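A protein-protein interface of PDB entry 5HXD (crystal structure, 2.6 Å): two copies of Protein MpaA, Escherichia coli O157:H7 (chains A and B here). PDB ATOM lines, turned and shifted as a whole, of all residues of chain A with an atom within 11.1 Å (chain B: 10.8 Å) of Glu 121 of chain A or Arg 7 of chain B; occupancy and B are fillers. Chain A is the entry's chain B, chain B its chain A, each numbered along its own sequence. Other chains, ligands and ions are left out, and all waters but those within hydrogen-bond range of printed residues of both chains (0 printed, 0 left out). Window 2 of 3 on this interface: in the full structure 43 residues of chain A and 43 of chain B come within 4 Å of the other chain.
The backbone carbonyl oxygen (O) of Ser 220 of chain B lies close to the side-chain amide oxygen (OD1) of Asn 116 of chain A (3.2 Å).
The backbone NH of Glu 221 of chain B lies within hydrogen-bond range of the side-chain amide oxygen of Asn 116 of chain A.
The guanidinium group (NE) of Arg 7 of chain B is in salt-bridge range of the side-chain carboxylate (OD2) of Asp 123 of chain A, 2.4 Å away.
N of Val 125 of chain A sits at hydrogen-bond distance from O of Ala 8 of chain B.
The guanidinium group (NH1) of Arg 7 of chain B sits at hydrogen-bond distance from the backbone carbonyl oxygen (O) of Ala 119 of chain A (3.3 Å).
The indole nitrogen (NE1) of Trp 115 of chain A sits close to the guanidinium group (NH1) of Arg 10 of chain B (3.5 Å).
O of Val 124 of chain A is in hydrogen-bond range of N of Tyr 113 of chain A, at 2.7 Å.
The guanidinium group (NE) of Arg 10 of chain B is in hydrogen-bond range of the backbone carbonyl oxygen (O) of Arg 5 of chain B, 2.9 Å away.
The backbone carbonyl oxygen (O) of Thr 111 of chain A sits at hydrogen-bond distance from the backbone NH (N) of Leu 126 of chain A, 2.8 Å away.
The side-chain sulfur of Cys 61 of chain B is in hydrogen-bond range of the side-chain hydroxyl of Ser 220 of chain B.
O of Tyr 113 of chain A sits at hydrogen-bond distance from N of Asp 123 of chain A (3.3 Å).
SG of Cys 61 of chain B sits at hydrogen-bond distance from NH2 of Arg 64 of chain B.
Among the printed residues, merely in contact across the chains: Trp 115 of chain A with Arg 7 of chain B, Trp 115 of chain A with Arg 64 of chain B, Trp 115 of chain A with Thr 65 of chain B, Trp 115 of chain A with Leu 224 of chain B, Glu 121 of chain A with Arg 7 of chain B, Asp 123 of chain A with Ala 8 of chain B, Val 124 of chain A with Arg 7 of chain B, Val 124 of chain A with Ala 8 of chain B, Val 124 of chain A with Arg 10 of chain B, Val 124 of chain A with Gly 11 of chain B, Val 125 of chain A with Gly 11 of chain B and Leu 126 of chain A with Gly 11 of chain B.
Glu 121 of chain A touches just one residue of chain B: Arg 7 (3.6 Å).
Arg 7 of chain B touches just these residues of chain A: Trp 115 (3.6 Å), Ala 119 (3.3 Å), Glu 121 (3.6 Å), Asp 123 (2.4 Å) and Val 124 (3.1 Å).
No residue of chain B comes within 4 Å of Arg 114 of chain A.
Glu 120 of chain A touches none of the printed residues of chain B.
Of chain B, only Arg 7 and Ala 8 come within 4 Å of Asp 123 of chain A.
Val 124 of chain A touches just these residues of chain B: Arg 7, Ala 8, Arg 10 and Gly 11.
No residue of chain A comes within 4 Å of Pro 6 of chain B.
Of chain A, only Trp 115 and Val 124 come within 4 Å of Arg 10 of chain B.
Of the printed residues of chain A, Leu 224 of chain B touches Trp 115 (3.5 Å).
Printed residues of chain B within 4 Å of Trp 115 of chain A: Arg 7 (3.6 Å), Arg 10 (3.4 Å), Arg 64 (3.9 Å), Thr 65 (3.4 Å) and Leu 224 (3.5 Å).
The nearest residue of chain B that does not touch Glu 121 of chain A is Ala 8 of chain B (7.7 Å).
Of the 17 printed residues of chain A, 8 touch a printed residue of chain B.
Hydrophobic or aromatic side chains of chain A within 4 Å of the printed part of chain B: Trp 115, Val 124, Val 125 and Leu 126.
Among the printed residues, Asp or Glu carboxylates within 4 Å of a Lys or Arg side-chain nitrogen of the other chain: Asp 123 of chain A with Arg 7 of chain B (2.4 Å).
No position is printed for both chains.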
ATOM      1  N   ARG A  89       0.545  -3.921 -20.533  1.00  0.00           N
ATOM      2  CA  ARG A  89       0.774  -3.090 -19.369  1.00  0.00           C
ATOM      3  C   ARG A  89       1.636  -1.845 -19.608  1.00  0.00           C
ATOM      4  O   ARG A  89       1.241  -0.742 -19.214  1.00  0.00           O
ATOM      5  CB  ARG A  89       1.410  -3.950 -18.276  1.00  0.00           C
ATOM      6  CG  ARG A  89       1.337  -3.338 -16.886  1.00  0.00           C
ATOM      7  CD  ARG A  89       1.889  -4.299 -15.860  1.00  0.00           C
ATOM      8  NE  ARG A  89       2.430  -3.604 -14.700  1.00  0.00           N
ATOM      9  CZ  ARG A  89       1.831  -3.535 -13.515  1.00  0.00           C
ATOM     10  NH1 ARG A  89       0.662  -4.138 -13.314  1.00  0.00           N
ATOM     11  NH2 ARG A  89       2.409  -2.865 -12.531  1.00  0.00           N
ATOM     12  N   THR A 111      11.660  -3.178 -13.296  1.00  0.00           N
ATOM     13  CA  THR A 111      10.492  -3.439 -12.461  1.00  0.00           C
ATOM     14  C   THR A 111      10.007  -4.828 -12.840  1.00  0.00           C
ATOM     15  O   THR A 111      10.405  -5.348 -13.885  1.00  0.00           O
ATOM     16  CB  THR A 111       9.362  -2.353 -12.646  1.00  0.00           C
ATOM     17  OG1 THR A 111       8.163  -2.751 -11.961  1.00  0.00           O
ATOM     18  CG2 THR A 111       9.044  -2.117 -14.119  1.00  0.00           C
ATOM     19  N   VAL A 112       9.195  -5.448 -11.987  1.00  0.00           N
ATOM     20  CA  VAL A 112       8.579  -6.737 -12.322  1.00  0.00           C
ATOM     21  C   VAL A 112       7.108  -6.726 -11.929  1.00  0.00           C
ATOM     22  O   VAL A 112       6.700  -5.932 -11.071  1.00  0.00           O
ATOM     23  CB  VAL A 112       9.289  -7.918 -11.633  1.00  0.00           C
ATOM     24  CG1 VAL A 112      10.536  -8.313 -12.410  1.00  0.00           C
ATOM     25  CG2 VAL A 112       9.625  -7.567 -10.189  1.00  0.00           C
ATOM     26  N   TYR A 113       6.306  -7.580 -12.564  1.00  0.00           N
ATOM     27  CA  TYR A 113       4.876  -7.602 -12.260  1.00  0.00           C
ATOM     28  C   TYR A 113       4.244  -8.971 -12.458  1.00  0.00           C
ATOM     29  O   TYR A 113       4.851  -9.877 -13.024  1.00  0.00           O
ATOM     30  CB  TYR A 113       4.126  -6.538 -13.088  1.00  0.00           C
ATOM     31  CG  TYR A 113       3.898  -6.819 -14.572  1.00  0.00           C
ATOM     32  CD1 TYR A 113       2.746  -7.467 -15.008  1.00  0.00           C
ATOM     33  CD2 TYR A 113       4.805  -6.384 -15.533  1.00  0.00           C
ATOM     34  CE1 TYR A 113       2.521  -7.714 -16.362  1.00  0.00           C
ATOM     35  CE2 TYR A 113       4.589  -6.620 -16.882  1.00  0.00           C
ATOM     36  CZ  TYR A 113       3.444  -7.283 -17.295  1.00  0.00           C
ATOM     37  OH  TYR A 113       3.224  -7.507 -18.643  1.00  0.00           O
ATOM     38  N   ARG A 114       3.020  -9.123 -11.967  1.00  0.00           N
ATOM     39  CA  ARG A 114       2.357 -10.418 -11.994  1.00  0.00           C
ATOM     40  C   ARG A 114       1.675 -10.708 -13.329  1.00  0.00           C
ATOM     41  O   ARG A 114       1.064  -9.827 -13.940  1.00  0.00           O
ATOM     42  CB  ARG A 114       1.346 -10.516 -10.849  1.00  0.00           C
ATOM     43  CG  ARG A 114       2.001 -10.505  -9.485  1.00  0.00           C
ATOM     44  CD  ARG A 114       1.013 -10.510  -8.334  1.00  0.00           C
ATOM     45  NE  ARG A 114       0.205 -11.721  -8.338  1.00  0.00           N
ATOM     46  CZ  ARG A 114      -0.770 -11.964  -7.472  1.00  0.00           C
ATOM     47  NH1 ARG A 114      -1.046 -11.079  -6.520  1.00  0.00           N
ATOM     48  NH2 ARG A 114      -1.460 -13.093  -7.549  1.00  0.00           N
ATOM     49  N   TRP A 115       1.790 -11.955 -13.775  1.00  0.00           N
ATOM     50  CA  TRP A 115       1.157 -12.386 -15.013  1.00  0.00           C
ATOM     51  C   TRP A 115      -0.378 -12.170 -14.893  1.00  0.00           C
ATOM     52  O   TRP A 115      -0.938 -11.404 -15.693  1.00  0.00           O
ATOM     53  CB  TRP A 115       1.570 -13.841 -15.338  1.00  0.00           C
ATOM     54  CG  TRP A 115       1.226 -14.302 -16.729  1.00  0.00           C
ATOM     55  CD1 TRP A 115       0.469 -15.392 -17.061  1.00  0.00           C
ATOM     56  CD2 TRP A 115       1.592 -13.676 -17.970  1.00  0.00           C
ATOM     57  NE1 TRP A 115       0.343 -15.486 -18.425  1.00  0.00           N
ATOM     58  CE2 TRP A 115       1.019 -14.448 -19.009  1.00  0.00           C
ATOM     59  CE3 TRP A 115       2.347 -12.546 -18.305  1.00  0.00           C
ATOM     60  CZ2 TRP A 115       1.178 -14.121 -20.364  1.00  0.00           C
ATOM     61  CZ3 TRP A 115       2.504 -12.223 -19.654  1.00  0.00           C
ATOM     62  CH2 TRP A 115       1.922 -13.011 -20.666  1.00  0.00           C
ATOM     63  N   ASN A 116      -1.053 -12.740 -13.886  1.00  0.00           N
ATOM     64  CA  ASN A 116      -2.451 -12.357 -13.684  1.00  0.00           C
ATOM     65  C   ASN A 116      -2.693 -12.436 -12.171  1.00  0.00           C
ATOM     66  O   ASN A 116      -1.744 -12.332 -11.384  1.00  0.00           O
ATOM     67  CB  ASN A 116      -3.502 -13.231 -14.456  1.00  0.00           C
ATOM     68  CG  ASN A 116      -2.899 -14.384 -15.329  1.00  0.00           C
ATOM     69  OD1 ASN A 116      -3.658 -15.066 -16.050  1.00  0.00           O
ATOM     70  ND2 ASN A 116      -1.678 -14.812 -15.005  1.00  0.00           N
ATOM     71  N   SER A 117      -3.942 -12.652 -11.766  1.00  0.00           N
ATOM     72  CA  SER A 117      -4.258 -12.889 -10.358  1.00  0.00           C
ATOM     73  C   SER A 117      -3.743 -14.258  -9.913  1.00  0.00           C
ATOM     74  O   SER A 117      -3.263 -14.434  -8.787  1.00  0.00           O
ATOM     75  CB  SER A 117      -5.765 -12.783 -10.121  1.00  0.00           C
ATOM     76  OG  SER A 117      -6.228 -11.519 -10.552  1.00  0.00           O
ATOM     77  N   ALA A 118      -3.812 -15.214 -10.835  1.00  0.00           N
ATOM     78  CA  ALA A 118      -3.355 -16.583 -10.595  1.00  0.00           C
ATOM     79  C   ALA A 118      -1.855 -16.758 -10.796  1.00  0.00           C
ATOM     80  O   ALA A 118      -1.378 -17.872 -11.020  1.00  0.00           O
ATOM     81  CB  ALA A 118      -4.113 -17.546 -11.503  1.00  0.00           C
ATOM     82  N   ALA A 119      -1.125 -15.654 -10.685  1.00  0.00           N
ATOM     83  CA  ALA A 119       0.280 -15.596 -11.059  1.00  0.00           C
ATOM     84  C   ALA A 119       1.258 -15.777  -9.928  1.00  0.00           C
ATOM     85  O   ALA A 119       2.409 -16.143 -10.197  1.00  0.00           O
ATOM     86  CB  ALA A 119       0.590 -14.264 -11.765  1.00  0.00           C
ATOM     87  N   GLU A 120       0.828 -15.521  -8.686  1.00  0.00           N
ATOM     88  CA  GLU A 120       1.612 -15.847  -7.470  1.00  0.00           C
ATOM     89  C   GLU A 120       2.863 -14.952  -7.312  1.00  0.00           C
ATOM     90  O   GLU A 120       2.994 -14.241  -6.319  1.00  0.00           O
ATOM     91  CB  GLU A 120       2.067 -17.323  -7.447  1.00  0.00           C
ATOM     92  CG  GLU A 120       1.258 -18.357  -8.288  1.00  0.00           C
ATOM     93  CD  GLU A 120       1.751 -19.724  -7.991  1.00  0.00           C
ATOM     94  OE1 GLU A 120       2.984 -19.836  -7.881  1.00  0.00           O
ATOM     95  OE2 GLU A 120       0.965 -20.674  -7.976  1.00  0.00           O
ATOM     96  N   GLU A 121       3.773 -14.962  -8.289  1.00  0.00           N
ATOM     97  CA  GLU A 121       5.059 -14.254  -8.148  1.00  0.00           C
ATOM     98  C   GLU A 121       5.269 -13.211  -9.242  1.00  0.00           C
ATOM     99  O   GLU A 121       5.143 -13.529 -10.433  1.00  0.00           O
ATOM    100  CB  GLU A 121       6.229 -15.247  -8.157  1.00  0.00           C
ATOM    101  CG  GLU A 121       6.173 -16.300  -7.047  1.00  0.00           C
ATOM    102  CD  GLU A 121       7.396 -17.217  -7.044  1.00  0.00           C
ATOM    103  OE1 GLU A 121       8.456 -16.810  -6.515  1.00  0.00           O
ATOM    104  OE2 GLU A 121       7.298 -18.345  -7.580  1.00  0.00           O
ATOM    105  N   ARG A 122       5.583 -11.978  -8.829  1.00  0.00           N
ATOM    106  CA  ARG A 122       5.869 -10.879  -9.752  1.00  0.00           C
ATOM    107  C   ARG A 122       7.173 -11.064 -10.515  1.00  0.00           C
ATOM    108  O   ARG A 122       8.194 -10.511 -10.121  1.00  0.00           O
ATOM    109  CB  ARG A 122       5.945  -9.547  -9.008  1.00  0.00           C
ATOM    110  CG  ARG A 122       4.749  -9.186  -8.163  1.00  0.00           C
ATOM    111  CD  ARG A 122       4.947  -7.820  -7.572  1.00  0.00           C
ATOM    112  NE  ARG A 122       6.296  -7.679  -7.035  1.00  0.00           N
ATOM    113  CZ  ARG A 122       6.745  -6.587  -6.427  1.00  0.00           C
ATOM    114  NH1 ARG A 122       5.944  -5.537  -6.278  1.00  0.00           N
ATOM    115  NH2 ARG A 122       7.991  -6.545  -5.966  1.00  0.00           N
ATOM    116  N   ASP A 123       7.133 -11.797 -11.620  1.00  0.00           N
ATOM    117  CA  ASP A 123       8.348 -12.158 -12.341  1.00  0.00           C
ATOM    118  C   ASP A 123       8.472 -11.463 -13.696  1.00  0.00           C
ATOM    119  O   ASP A 123       9.584 -11.210 -14.165  1.00  0.00           O
ATOM    120  CB  ASP A 123       8.389 -13.670 -12.538  1.00  0.00           C
ATOM    121  CG  ASP A 123       7.115 -14.201 -13.161  1.00  0.00           C
ATOM    122  OD1 ASP A 123       6.094 -13.483 -13.126  1.00  0.00           O
ATOM    123  OD2 ASP A 123       7.128 -15.334 -13.683  1.00  0.00           O
ATOM    124  N   VAL A 124       7.334 -11.168 -14.324  1.00  0.00           N
ATOM    125  CA  VAL A 124       7.313 -10.530 -15.643  1.00  0.00           C
ATOM    126  C   VAL A 124       7.953  -9.143 -15.586  1.00  0.00           C
ATOM    127  O   VAL A 124       7.471  -8.248 -14.893  1.00  0.00           O
ATOM    128  CB  VAL A 124       5.874 -10.419 -16.206  1.00  0.00           C
ATOM    129  CG1 VAL A 124       5.908 -10.112 -17.696  1.00  0.00           C
ATOM    130  CG2 VAL A 124       5.096 -11.704 -15.961  1.00  0.00           C
ATOM    131  N   VAL A 125       9.045  -8.981 -16.330  1.00  0.00           N
ATOM    132  CA  VAL A 125       9.934  -7.820 -16.229  1.00  0.00           C
ATOM    133  C   VAL A 125       9.527  -6.643 -17.125  1.00  0.00           C
ATOM    134  O   VAL A 125       9.024  -6.835 -18.224  1.00  0.00           O
ATOM    135  CB  VAL A 125      11.396  -8.249 -16.565  1.00  0.00           C
ATOM    136  CG1 VAL A 125      12.364  -7.065 -16.581  1.00  0.00           C
ATOM    137  CG2 VAL A 125      11.860  -9.316 -15.588  1.00  0.00           C
ATOM    138  N   LEU A 126       9.715  -5.423 -16.626  1.00  0.00           N
ATOM    139  CA  LEU A 126       9.610  -4.218 -17.449  1.00  0.00           C
ATOM    140  C   LEU A 126      10.736  -3.282 -17.044  1.00  0.00           C
ATOM    141  O   LEU A 126      11.493  -3.582 -16.121  1.00  0.00           O
ATOM    142  CB  LEU A 126       8.248  -3.515 -17.289  1.00  0.00           C
ATOM    143  CG  LEU A 126       6.921  -4.227 -17.588  1.00  0.00           C
ATOM    144  CD1 LEU A 126       5.752  -3.324 -17.263  1.00  0.00           C
ATOM    145  CD2 LEU A 126       6.848  -4.696 -19.043  1.00  0.00           C
ATOM    146  N   THR B   2      11.348 -24.941 -25.833  1.00  0.00           N
ATOM    147  CA  THR B   2      10.050 -24.791 -25.142  1.00  0.00           C
ATOM    148  C   THR B   2       8.902 -24.293 -26.039  1.00  0.00           C
ATOM    149  O   THR B   2       9.111 -23.494 -26.954  1.00  0.00           O
ATOM    150  CB  THR B   2      10.166 -23.795 -23.935  1.00  0.00           C
ATOM    151  OG1 THR B   2      11.325 -24.100 -23.153  1.00  0.00           O
ATOM    152  CG2 THR B   2       8.938 -23.859 -23.037  1.00  0.00           C
ATOM    153  N   VAL B   3       7.685 -24.754 -25.756  1.00  0.00           N
ATOM    154  CA  VAL B   3       6.489 -24.273 -26.458  1.00  0.00           C
ATOM    155  C   VAL B   3       6.181 -22.785 -26.146  1.00  0.00           C
ATOM    156  O   VAL B   3       5.560 -22.086 -26.953  1.00  0.00           O
ATOM    157  CB  VAL B   3       5.234 -25.155 -26.108  1.00  0.00           C
ATOM    158  CG1 VAL B   3       4.149 -25.035 -27.181  1.00  0.00           C
ATOM    159  CG2 VAL B   3       5.626 -26.618 -25.896  1.00  0.00           C
ATOM    160  N   THR B   4       6.619 -22.305 -24.977  1.00  0.00           N
ATOM    161  CA  THR B   4       6.339 -20.928 -24.535  1.00  0.00           C
ATOM    162  C   THR B   4       7.560 -20.186 -23.982  1.00  0.00           C
ATOM    163  O   THR B   4       8.363 -20.766 -23.250  1.00  0.00           O
ATOM    164  CB  THR B   4       5.261 -20.893 -23.429  1.00  0.00           C
ATOM    165  OG1 THR B   4       5.850 -21.248 -22.167  1.00  0.00           O
ATOM    166  CG2 THR B   4       4.106 -21.833 -23.753  1.00  0.00           C
ATOM    167  N   ARG B   5       7.681 -18.905 -24.322  1.00  0.00           N
ATOM    168  CA  ARG B   5       8.643 -18.012 -23.669  1.00  0.00           C
ATOM    169  C   ARG B   5       8.450 -18.020 -22.143  1.00  0.00           C
ATOM    170  O   ARG B   5       7.320 -18.127 -21.658  1.00  0.00           O
ATOM    171  CB  ARG B   5       8.500 -16.581 -24.197  1.00  0.00           C
ATOM    172  CG  ARG B   5       8.869 -16.383 -25.651  1.00  0.00           C
ATOM    173  CD  ARG B   5       9.274 -14.921 -25.928  1.00  0.00           C
ATOM    174  NE  ARG B   5       8.177 -13.980 -25.692  1.00  0.00           N
ATOM    175  CZ  ARG B   5       8.286 -12.654 -25.737  1.00  0.00           C
ATOM    176  NH1 ARG B   5       9.450 -12.075 -25.993  1.00  0.00           N
ATOM    177  NH2 ARG B   5       7.219 -11.903 -25.520  1.00  0.00           N
ATOM    178  N   PRO B   6       9.552 -17.912 -21.382  1.00  0.00           N
ATOM    179  CA  PRO B   6       9.478 -17.831 -19.915  1.00  0.00           C
ATOM    180  C   PRO B   6       8.615 -16.651 -19.454  1.00  0.00           C
ATOM    181  O   PRO B   6       8.740 -15.551 -20.004  1.00  0.00           O
ATOM    182  CB  PRO B   6      10.940 -17.627 -19.492  1.00  0.00           C
ATOM    183  CG  PRO B   6      11.743 -18.142 -20.617  1.00  0.00           C
ATOM    184  CD  PRO B   6      10.942 -17.886 -21.867  1.00  0.00           C
ATOM    185  N   ARG B   7       7.762 -16.885 -18.456  1.00  0.00           N
ATOM    186  CA  ARG B   7       6.825 -15.877 -17.953  1.00  0.00           C
ATOM    187  C   ARG B   7       7.513 -14.556 -17.643  1.00  0.00           C
ATOM    188  O   ARG B   7       6.919 -13.494 -17.801  1.00  0.00           O
ATOM    189  CB  ARG B   7       6.110 -16.398 -16.703  1.00  0.00           C
ATOM    190  CG  ARG B   7       4.829 -15.656 -16.344  1.00  0.00           C
ATOM    191  CD  ARG B   7       4.115 -16.336 -15.179  1.00  0.00           C
ATOM    192  NE  ARG B   7       4.904 -16.287 -13.947  1.00  0.00           N
ATOM    193  CZ  ARG B   7       4.617 -16.971 -12.842  1.00  0.00           C
ATOM    194  NH1 ARG B   7       3.554 -17.765 -12.813  1.00  0.00           N
ATOM    195  NH2 ARG B   7       5.393 -16.865 -11.768  1.00  0.00           N
ATOM    196  N   ALA B   8       8.776 -14.629 -17.230  1.00  0.00           N
ATOM    197  CA  ALA B   8       9.530 -13.450 -16.817  1.00  0.00           C
ATOM    198  C   ALA B   8       9.842 -12.471 -17.951  1.00  0.00           C
ATOM    199  O   ALA B   8      10.166 -11.322 -17.687  1.00  0.00           O
ATOM    200  CB  ALA B   8      10.821 -13.882 -16.143  1.00  0.00           C
ATOM    201  N   GLU B   9       9.758 -12.905 -19.204  1.00  0.00           N
ATOM    202  CA  GLU B   9      10.110 -12.015 -20.314  1.00  0.00           C
ATOM    203  C   GLU B   9       8.956 -11.724 -21.275  1.00  0.00           C
ATOM    204  O   GLU B   9       9.165 -11.168 -22.355  1.00  0.00           O
ATOM    205  CB  GLU B   9      11.303 -12.580 -21.089  1.00  0.00           C
ATOM    206  CG  GLU B   9      11.108 -14.004 -21.629  1.00  0.00           C
ATOM    207  CD  GLU B   9      12.348 -14.548 -22.334  1.00  0.00           C
ATOM    208  OE1 GLU B   9      12.731 -14.005 -23.394  1.00  0.00           O
ATOM    209  OE2 GLU B   9      12.954 -15.501 -21.805  1.00  0.00           O
ATOM    210  N   ARG B  10       7.738 -12.053 -20.863  1.00  0.00           N
ATOM    211  CA  ARG B  10       6.567 -11.796 -21.689  1.00  0.00           C
ATOM    212  C   ARG B  10       6.073 -10.338 -21.585  1.00  0.00           C
ATOM    213  O   ARG B  10       4.924 -10.032 -21.901  1.00  0.00           O
ATOM    214  CB  ARG B  10       5.449 -12.777 -21.312  1.00  0.00           C
ATOM    215  CG  ARG B  10       5.809 -14.269 -21.496  1.00  0.00           C
ATOM    216  CD  ARG B  10       4.708 -15.147 -20.916  1.00  0.00           C
ATOM    217  NE  ARG B  10       4.934 -16.581 -21.053  1.00  0.00           N
ATOM    218  CZ  ARG B  10       4.181 -17.500 -20.451  1.00  0.00           C
ATOM    219  NH1 ARG B  10       3.175 -17.114 -19.677  1.00  0.00           N
ATOM    220  NH2 ARG B  10       4.426 -18.796 -20.607  1.00  0.00           N
ATOM    221  N   GLY B  11       6.943  -9.433 -21.151  1.00  0.00           N
ATOM    222  CA  GLY B  11       6.568  -8.036 -21.039  1.00  0.00           C
ATOM    223  C   GLY B  11       6.688  -7.261 -22.342  1.00  0.00           C
ATOM    224  O   GLY B  11       6.037  -6.226 -22.535  1.00  0.00           O
ATOM    225  N   ALA B  12       7.536  -7.744 -23.241  1.00  0.00           N
ATOM    226  CA  ALA B  12       7.701  -7.083 -24.526  1.00  0.00           C
ATOM    227  C   ALA B  12       7.229  -7.995 -25.641  1.00  0.00           C
ATOM    228  O   ALA B  12       6.867  -9.151 -25.400  1.00  0.00           O
ATOM    229  CB  ALA B  12       9.147  -6.669 -24.744  1.00  0.00           C
ATOM    230  N   CYS B  61      -1.233 -11.421 -25.261  1.00  0.00           N
ATOM    231  CA  CYS B  61      -0.557 -12.297 -24.304  1.00  0.00           C
ATOM    232  C   CYS B  61      -0.089 -13.554 -25.007  1.00  0.00           C
ATOM    233  O   CYS B  61       1.032 -14.017 -24.799  1.00  0.00           O
ATOM    234  CB  CYS B  61      -1.476 -12.658 -23.136  1.00  0.00           C
ATOM    235  SG  CYS B  61      -1.631 -11.356 -21.880  1.00  0.00           S
ATOM    236  N   ARG B  64       2.799 -12.859 -27.156  1.00  0.00           N
ATOM    237  CA  ARG B  64       3.981 -12.597 -26.323  1.00  0.00           C
ATOM    238  C   ARG B  64       4.427 -13.847 -25.548  1.00  0.00           C
ATOM    239  O   ARG B  64       5.475 -13.834 -24.895  1.00  0.00           O
ATOM    240  CB  ARG B  64       3.704 -11.434 -25.333  1.00  0.00           C
ATOM    241  CG  ARG B  64       3.794 -10.027 -25.951  1.00  0.00           C
ATOM    242  CD  ARG B  64       3.552  -8.881 -24.953  1.00  0.00           C
ATOM    243  NE  ARG B  64       2.156  -8.813 -24.505  1.00  0.00           N
ATOM    244  CZ  ARG B  64       1.743  -9.046 -23.260  1.00  0.00           C
ATOM    245  NH1 ARG B  64       2.619  -9.351 -22.317  1.00  0.00           N
ATOM    246  NH2 ARG B  64       0.450  -8.979 -22.965  1.00  0.00           N
ATOM    247  N   THR B  65       3.630 -14.916 -25.622  1.00  0.00           N
ATOM    248  CA  THR B  65       3.883 -16.157 -24.879  1.00  0.00           C
ATOM    249  C   THR B  65       4.463 -17.260 -25.752  1.00  0.00           C
ATOM    250  O   THR B  65       5.589 -17.704 -25.532  1.00  0.00           O
ATOM    251  CB  THR B  65       2.598 -16.696 -24.234  1.00  0.00           C
ATOM    252  OG1 THR B  65       2.196 -15.816 -23.180  1.00  0.00           O
ATOM    253  CG2 THR B  65       2.812 -18.095 -23.667  1.00  0.00           C
ATOM    254  N   LEU B  66       3.671 -17.705 -26.728  1.00  0.00           N
ATOM    255  CA  LEU B  66       4.069 -18.730 -27.689  1.00  0.00           C
ATOM    256  C   LEU B  66       5.456 -18.430 -28.259  1.00  0.00           C
ATOM    257  O   LEU B  66       5.808 -17.270 -28.466  1.00  0.00           O
ATOM    258  CB  LEU B  66       3.029 -18.838 -28.813  1.00  0.00           C
ATOM    259  CG  LEU B  66       3.356 -19.843 -29.939  1.00  0.00           C
ATOM    260  CD1 LEU B  66       3.549 -21.261 -29.387  1.00  0.00           C
ATOM    261  CD2 LEU B  66       2.314 -19.808 -31.068  1.00  0.00           C
ATOM    262  N   THR B  67       6.256 -19.473 -28.475  1.00  0.00           N
ATOM    263  CA  THR B  67       7.608 -19.276 -28.973  1.00  0.00           C
ATOM    264  C   THR B  67       7.496 -18.860 -30.429  1.00  0.00           C
ATOM    265  O   THR B  67       6.764 -19.488 -31.187  1.00  0.00           O
ATOM    266  CB  THR B  67       8.459 -20.537 -28.814  1.00  0.00           C
ATOM    267  OG1 THR B  67       8.300 -21.041 -27.480  1.00  0.00           O
ATOM    268  CG2 THR B  67       9.935 -20.230 -29.074  1.00  0.00           C
ATOM    269  N   SER B 220      -6.688 -13.960 -19.611  1.00  0.00           N
ATOM    270  CA  SER B 220      -5.246 -14.156 -19.716  1.00  0.00           C
ATOM    271  C   SER B 220      -4.802 -15.441 -18.992  1.00  0.00           C
ATOM    272  O   SER B 220      -3.662 -15.883 -19.140  1.00  0.00           O
ATOM    273  CB  SER B 220      -4.514 -12.943 -19.154  1.00  0.00           C
ATOM    274  OG  SER B 220      -3.135 -13.024 -19.445  1.00  0.00           O
ATOM    275  N   GLU B 221      -5.723 -16.011 -18.210  1.00  0.00           N
ATOM    276  CA  GLU B 221      -5.583 -17.308 -17.532  1.00  0.00           C
ATOM    277  C   GLU B 221      -6.331 -18.420 -18.299  1.00  0.00           C
ATOM    278  O   GLU B 221      -5.733 -19.374 -18.795  1.00  0.00           O
ATOM    279  CB  GLU B 221      -6.104 -17.184 -16.073  1.00  0.00           C
ATOM    280  CG  GLU B 221      -6.693 -18.438 -15.369  1.00  0.00           C
ATOM    281  CD  GLU B 221      -5.811 -19.694 -15.414  1.00  0.00           C
ATOM    282  OE1 GLU B 221      -4.568 -19.567 -15.547  1.00  0.00           O
ATOM    283  OE2 GLU B 221      -6.371 -20.818 -15.321  1.00  0.00           O
ATOM    284  N   LEU B 224      -5.646 -18.577 -22.577  1.00  0.00           N
ATOM    285  CA  LEU B 224      -4.307 -18.333 -23.101  1.00  0.00           C
ATOM    286  C   LEU B 224      -3.808 -19.579 -23.790  1.00  0.00           C
ATOM    287  O   LEU B 224      -3.062 -19.494 -24.758  1.00  0.00           O
ATOM    288  CB  LEU B 224      -3.352 -17.906 -21.984  1.00  0.00           C
ATOM    289  CG  LEU B 224      -1.911 -17.540 -22.358  1.00  0.00           C
ATOM    290  CD1 LEU B 224      -1.879 -16.734 -23.635  1.00  0.00           C
ATOM    291  CD2 LEU B 224      -1.235 -16.763 -21.227  1.00  0.00           C
